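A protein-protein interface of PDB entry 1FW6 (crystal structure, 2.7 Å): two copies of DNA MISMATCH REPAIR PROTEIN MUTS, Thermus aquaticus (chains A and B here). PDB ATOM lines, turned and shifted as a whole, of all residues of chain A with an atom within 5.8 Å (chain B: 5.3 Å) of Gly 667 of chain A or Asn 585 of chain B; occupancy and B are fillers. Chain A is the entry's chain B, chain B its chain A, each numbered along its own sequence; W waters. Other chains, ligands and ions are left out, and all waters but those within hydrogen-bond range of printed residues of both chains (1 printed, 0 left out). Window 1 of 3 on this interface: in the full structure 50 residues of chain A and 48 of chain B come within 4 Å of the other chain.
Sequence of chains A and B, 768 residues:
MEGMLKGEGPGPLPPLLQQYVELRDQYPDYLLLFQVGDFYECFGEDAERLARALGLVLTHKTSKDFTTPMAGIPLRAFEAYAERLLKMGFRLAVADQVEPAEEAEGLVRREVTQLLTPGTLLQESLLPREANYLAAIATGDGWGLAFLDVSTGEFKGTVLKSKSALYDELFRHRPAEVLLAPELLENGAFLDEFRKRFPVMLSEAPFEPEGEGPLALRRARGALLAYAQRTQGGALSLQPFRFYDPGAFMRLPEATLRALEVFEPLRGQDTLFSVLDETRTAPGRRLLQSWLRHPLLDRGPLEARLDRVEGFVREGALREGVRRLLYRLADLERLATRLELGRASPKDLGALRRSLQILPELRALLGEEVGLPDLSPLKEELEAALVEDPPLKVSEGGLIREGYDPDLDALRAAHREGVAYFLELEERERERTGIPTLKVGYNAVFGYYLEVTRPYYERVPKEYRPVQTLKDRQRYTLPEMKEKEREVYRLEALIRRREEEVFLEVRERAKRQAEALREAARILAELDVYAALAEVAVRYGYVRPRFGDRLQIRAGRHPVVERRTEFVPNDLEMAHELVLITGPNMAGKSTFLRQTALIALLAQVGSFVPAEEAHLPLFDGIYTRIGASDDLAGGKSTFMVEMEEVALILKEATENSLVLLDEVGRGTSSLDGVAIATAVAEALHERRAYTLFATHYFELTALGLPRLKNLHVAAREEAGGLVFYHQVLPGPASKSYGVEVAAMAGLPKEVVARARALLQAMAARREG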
ATOM      1  N   SER A 637      16.483  -1.777  14.966  1.00  0.00           N
ATOM      2  CA  SER A 637      16.312  -0.520  14.248  1.00  0.00           C
ATOM      3  C   SER A 637      14.900  -0.027  14.548  1.00  0.00           C
ATOM      4  O   SER A 637      14.035  -0.819  14.926  1.00  0.00           O
ATOM      5  CB  SER A 637      16.482  -0.731  12.736  1.00  0.00           C
ATOM      6  OG  SER A 637      15.393  -1.440  12.161  1.00  0.00           O
ATOM      7  N   PHE A 639      12.780   0.866  12.508  1.00  0.00           N
ATOM      8  CA  PHE A 639      11.977   0.222  11.487  1.00  0.00           C
ATOM      9  C   PHE A 639      11.452  -1.129  11.983  1.00  0.00           C
ATOM     10  O   PHE A 639      10.253  -1.384  11.958  1.00  0.00           O
ATOM     11  CB  PHE A 639      12.818   0.021  10.220  1.00  0.00           C
ATOM     12  CG  PHE A 639      12.054  -0.558   9.082  1.00  0.00           C
ATOM     13  CD1 PHE A 639      11.064   0.184   8.449  1.00  0.00           C
ATOM     14  CD2 PHE A 639      12.284  -1.865   8.670  1.00  0.00           C
ATOM     15  CE1 PHE A 639      10.305  -0.371   7.417  1.00  0.00           C
ATOM     16  CE2 PHE A 639      11.530  -2.436   7.639  1.00  0.00           C
ATOM     17  CZ  PHE A 639      10.537  -1.688   7.013  1.00  0.00           C
ATOM     18  N   GLY A 665       5.960   2.904   7.247  1.00  0.00           N
ATOM     19  CA  GLY A 665       6.759   2.773   6.048  1.00  0.00           C
ATOM     20  C   GLY A 665       8.099   3.453   6.230  1.00  0.00           C
ATOM     21  O   GLY A 665       9.095   3.081   5.627  1.00  0.00           O
ATOM     22  N   ARG A 666       8.134   4.454   7.085  1.00  0.00           N
ATOM     23  CA  ARG A 666       9.372   5.164   7.314  1.00  0.00           C
ATOM     24  C   ARG A 666      10.455   4.289   7.930  1.00  0.00           C
ATOM     25  O   ARG A 666      10.197   3.170   8.383  1.00  0.00           O
ATOM     26  CB  ARG A 666       9.124   6.354   8.232  1.00  0.00           C
ATOM     27  CG  ARG A 666       8.744   5.978   9.638  1.00  0.00           C
ATOM     28  CD  ARG A 666       8.744   7.219  10.510  1.00  0.00           C
ATOM     29  NE  ARG A 666       8.089   7.013  11.797  1.00  0.00           N
ATOM     30  CZ  ARG A 666       7.794   7.993  12.643  1.00  0.00           C
ATOM     31  NH1 ARG A 666       8.105   9.243  12.326  1.00  0.00           N
ATOM     32  NH2 ARG A 666       7.180   7.730  13.795  1.00  0.00           N
ATOM     33  N   GLY A 667      11.677   4.809   7.944  1.00  0.00           N
ATOM     34  CA  GLY A 667      12.769   4.092   8.558  1.00  0.00           C
ATOM     35  C   GLY A 667      13.569   3.170   7.682  1.00  0.00           C
ATOM     36  O   GLY A 667      14.346   2.379   8.193  1.00  0.00           O
ATOM     37  N   THR A 668      13.406   3.262   6.374  1.00  0.00           N
ATOM     38  CA  THR A 668      14.169   2.400   5.483  1.00  0.00           C
ATOM     39  C   THR A 668      14.315   3.029   4.102  1.00  0.00           C
ATOM     40  O   THR A 668      14.254   4.258   3.966  1.00  0.00           O
ATOM     41  CB  THR A 668      13.503   1.021   5.359  1.00  0.00           C
ATOM     42  OG1 THR A 668      14.186   0.253   4.365  1.00  0.00           O
ATOM     43  CG2 THR A 668      12.039   1.163   5.000  1.00  0.00           C
ATOM     44  N   SER A 669      14.534   2.194   3.088  1.00  0.00           N
ATOM     45  CA  SER A 669      14.670   2.668   1.708  1.00  0.00           C
ATOM     46  C   SER A 669      13.364   3.324   1.300  1.00  0.00           C
ATOM     47  O   SER A 669      12.328   3.055   1.895  1.00  0.00           O
ATOM     48  CB  SER A 669      14.962   1.493   0.770  1.00  0.00           C
ATOM     49  OG  SER A 669      14.896   1.890  -0.588  1.00  0.00           O
ATOM     50  N   TYR A 697       3.702   9.129   1.613  1.00  0.00           N
ATOM     51  CA  TYR A 697       3.743   8.478   0.315  1.00  0.00           C
ATOM     52  C   TYR A 697       2.458   8.838  -0.434  1.00  0.00           C
ATOM     53  O   TYR A 697       1.402   8.243  -0.204  1.00  0.00           O
ATOM     54  CB  TYR A 697       3.848   6.956   0.482  1.00  0.00           C
ATOM     55  CG  TYR A 697       5.083   6.504   1.228  1.00  0.00           C
ATOM     56  CD1 TYR A 697       4.984   5.657   2.344  1.00  0.00           C
ATOM     57  CD2 TYR A 697       6.348   6.936   0.838  1.00  0.00           C
ATOM     58  CE1 TYR A 697       6.116   5.262   3.056  1.00  0.00           C
ATOM     59  CE2 TYR A 697       7.487   6.546   1.539  1.00  0.00           C
ATOM     60  CZ  TYR A 697       7.366   5.712   2.649  1.00  0.00           C
ATOM     61  OH  TYR A 697       8.497   5.365   3.359  1.00  0.00           O
ATOM     62  N   GLY B 583      23.943   0.490   3.590  1.00  0.00           N
ATOM     63  CA  GLY B 583      23.814  -0.867   4.080  1.00  0.00           C
ATOM     64  C   GLY B 583      22.691  -0.957   5.093  1.00  0.00           C
ATOM     65  O   GLY B 583      22.286   0.044   5.691  1.00  0.00           O
ATOM     66  N   PRO B 584      22.187  -2.166   5.331  1.00  0.00           N
ATOM     67  CA  PRO B 584      21.092  -2.456   6.262  1.00  0.00           C
ATOM     68  C   PRO B 584      21.213  -1.952   7.696  1.00  0.00           C
ATOM     69  O   PRO B 584      22.281  -1.995   8.289  1.00  0.00           O
ATOM     70  CB  PRO B 584      20.999  -3.976   6.195  1.00  0.00           C
ATOM     71  CG  PRO B 584      22.416  -4.373   5.946  1.00  0.00           C
ATOM     72  CD  PRO B 584      22.847  -3.408   4.898  1.00  0.00           C
ATOM     73  N   ASN B 585      20.099  -1.486   8.256  1.00  0.00           N
ATOM     74  CA  ASN B 585      20.087  -1.020   9.635  1.00  0.00           C
ATOM     75  C   ASN B 585      20.355  -2.199  10.584  1.00  0.00           C
ATOM     76  O   ASN B 585      20.019  -3.350  10.285  1.00  0.00           O
ATOM     77  CB  ASN B 585      18.752  -0.344   9.946  1.00  0.00           C
ATOM     78  CG  ASN B 585      18.690   1.094   9.418  1.00  0.00           C
ATOM     79  OD1 ASN B 585      17.619   1.687   9.308  1.00  0.00           O
ATOM     80  ND2 ASN B 585      19.846   1.657   9.106  1.00  0.00           N
ATOM     81  N   MET B 586      20.966  -1.898  11.727  1.00  0.00           N
ATOM     82  CA  MET B 586      21.355  -2.898  12.713  1.00  0.00           C
ATOM     83  C   MET B 586      22.711  -3.476  12.293  1.00  0.00           C
ATOM     84  O   MET B 586      23.308  -4.280  13.000  1.00  0.00           O
ATOM     85  CB  MET B 586      20.315  -4.013  12.828  1.00  0.00           C
ATOM     86  CG  MET B 586      19.064  -3.610  13.589  1.00  0.00           C
ATOM     87  SD  MET B 586      17.652  -4.953  13.535  1.00  0.00           S
ATOM     88  CE  MET B 586      17.001  -4.678  11.746  1.00  0.00           C
ATOM     89  N   ALA B 587      23.209  -3.032  11.143  1.00  0.00           N
ATOM     90  CA  ALA B 587      24.483  -3.521  10.638  1.00  0.00           C
ATOM     91  C   ALA B 587      25.710  -2.807  11.188  1.00  0.00           C
ATOM     92  O   ALA B 587      26.746  -3.444  11.348  1.00  0.00           O
ATOM     93  CB  ALA B 587      24.495  -3.481   9.114  1.00  0.00           C
ATOM     94  N   LYS B 589      26.334   1.200  10.679  1.00  0.00           N
ATOM     95  CA  LYS B 589      26.539   2.572  10.209  1.00  0.00           C
ATOM     96  C   LYS B 589      26.747   3.648  11.269  1.00  0.00           C
ATOM     97  O   LYS B 589      27.774   4.320  11.278  1.00  0.00           O
ATOM     98  CB  LYS B 589      25.385   2.985   9.316  1.00  0.00           C
ATOM     99  CG  LYS B 589      25.406   2.342   7.951  1.00  0.00           C
ATOM    100  CD  LYS B 589      24.111   2.595   7.217  1.00  0.00           C
ATOM    101  CE  LYS B 589      22.978   1.922   7.945  1.00  0.00           C
ATOM    102  NZ  LYS B 589      21.785   1.867   7.093  1.00  0.00           N
ATOM    103  N   GLU B 663      21.753   9.834   8.352  1.00  0.00           N
ATOM    104  CA  GLU B 663      20.416   9.861   7.769  1.00  0.00           C
ATOM    105  C   GLU B 663      19.840  11.239   7.431  1.00  0.00           C
ATOM    106  O   GLU B 663      18.615  11.381   7.351  1.00  0.00           O
ATOM    107  CB  GLU B 663      19.432   9.152   8.712  1.00  0.00           C
ATOM    108  CG  GLU B 663      19.939   7.871   9.371  1.00  0.00           C
ATOM    109  CD  GLU B 663      20.123   6.727   8.390  1.00  0.00           C
ATOM    110  OE1 GLU B 663      19.890   6.931   7.179  1.00  0.00           O
ATOM    111  OE2 GLU B 663      20.505   5.620   8.834  1.00  0.00           O
ATOM    112  N   HIS B 696      20.278   6.372   3.408  1.00  0.00           N
ATOM    113  CA  HIS B 696      19.451   5.302   2.852  1.00  0.00           C
ATOM    114  C   HIS B 696      19.091   5.626   1.390  1.00  0.00           C
ATOM    115  O   HIS B 696      18.425   4.840   0.706  1.00  0.00           O
ATOM    116  CB  HIS B 696      18.192   5.095   3.682  1.00  0.00           C
ATOM    117  CG  HIS B 696      18.378   4.128   4.803  1.00  0.00           C
ATOM    118  ND1 HIS B 696      19.097   4.434   5.937  1.00  0.00           N
ATOM    119  CD2 HIS B 696      17.996   2.836   4.938  1.00  0.00           C
ATOM    120  CE1 HIS B 696      19.152   3.372   6.723  1.00  0.00           C
ATOM    121  NE2 HIS B 696      18.492   2.389   6.138  1.00  0.00           N
ATOM    122  N   PHE B 724      23.293  -9.926  10.672  1.00  0.00           N
ATOM    123  CA  PHE B 724      24.085  -8.740  10.393  1.00  0.00           C
ATOM    124  C   PHE B 724      25.520  -8.846  10.907  1.00  0.00           C
ATOM    125  O   PHE B 724      25.763  -9.038  12.109  1.00  0.00           O
ATOM    126  CB  PHE B 724      23.431  -7.501  11.008  1.00  0.00           C
ATOM    127  CG  PHE B 724      22.020  -7.284  10.568  1.00  0.00           C
ATOM    128  CD1 PHE B 724      20.976  -7.895  11.234  1.00  0.00           C
ATOM    129  CD2 PHE B 724      21.741  -6.467   9.484  1.00  0.00           C
ATOM    130  CE1 PHE B 724      19.669  -7.691  10.834  1.00  0.00           C
ATOM    131  CE2 PHE B 724      20.444  -6.259   9.075  1.00  0.00           C
ATOM    132  CZ  PHE B 724      19.400  -6.874   9.752  1.00  0.00           C
HETATM  133  O   HOH W   1      15.651   0.122   8.402  1.00  0.00           O
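Along chain A the printed residues that touch a printed residue of chain B span positions 637 to 669. Of the 9 printed residues of chain B, 3 touch a printed residue of chain A. Printed residues of chain B that touch a printed residue of chain A: Asn 585, Met 586 and His 696. Among the printed residues, no Asp or Glu carboxylate lies within 4 Å of a Lys or Arg side-chain nitrogen of the other chain.
Ser 637 of chain A touches Asn 585 of chain B. Asn 585 of chain B touches Gly 667 of chain A (OD1 to O, 3.5 Å). Thr 668 of chain A touches His 696 of chain B. His 696 of chain B touches Ser 669 of chain A (CD2 to N, 3.98 Å).
NZ of Lys 589 of chain B sits close to ND2 of Asn 585 of chain B, at 2.8 Å. ND2 of Asn 585 of chain B lies close to NE2 of His 696 of chain B (3.3 Å). NZ of Lys 589 of chain B sits close to NE2 of His 696 of chain B (3.5 Å). ND1 of His 696 of chain B lies within hydrogen-bond range of OE1 of Glu 663 of chain B (2.9 Å).
The side-chain sulfur (SD) of Met 586 of chain B lies close to the backbone NH (N) of Ser 637 of chain A.
Gly 665 of chain A touches none of the printed residues of chain B. Gly 667 of chain A touches just one residue of chain B: Asn 585 (3.5 Å). Of the printed residues of chain B, Thr 668 of chain A touches His 696 (3.8 Å). Asn 585 of chain B touches two residues of chain A. Glu 663 of chain B touches none of the printed residues of chain A. Of the printed residues of chain A, His 696 of chain B touches Thr 668 and Ser 669. The nearest residue of chain B that does not touch Gly 667 of chain A is His 696 of chain B (4.6 Å). The nearest printed residue of chain A that does not touch His 696 of chain B is Gly 667 of chain A (4.6 Å).
No position is printed for both chains.
Water W1 lies within hydrogen-bond range of O of Gly 667 of chain A (2.6 Å) and OD1 of Asn 585 of chain B (2.7 Å).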
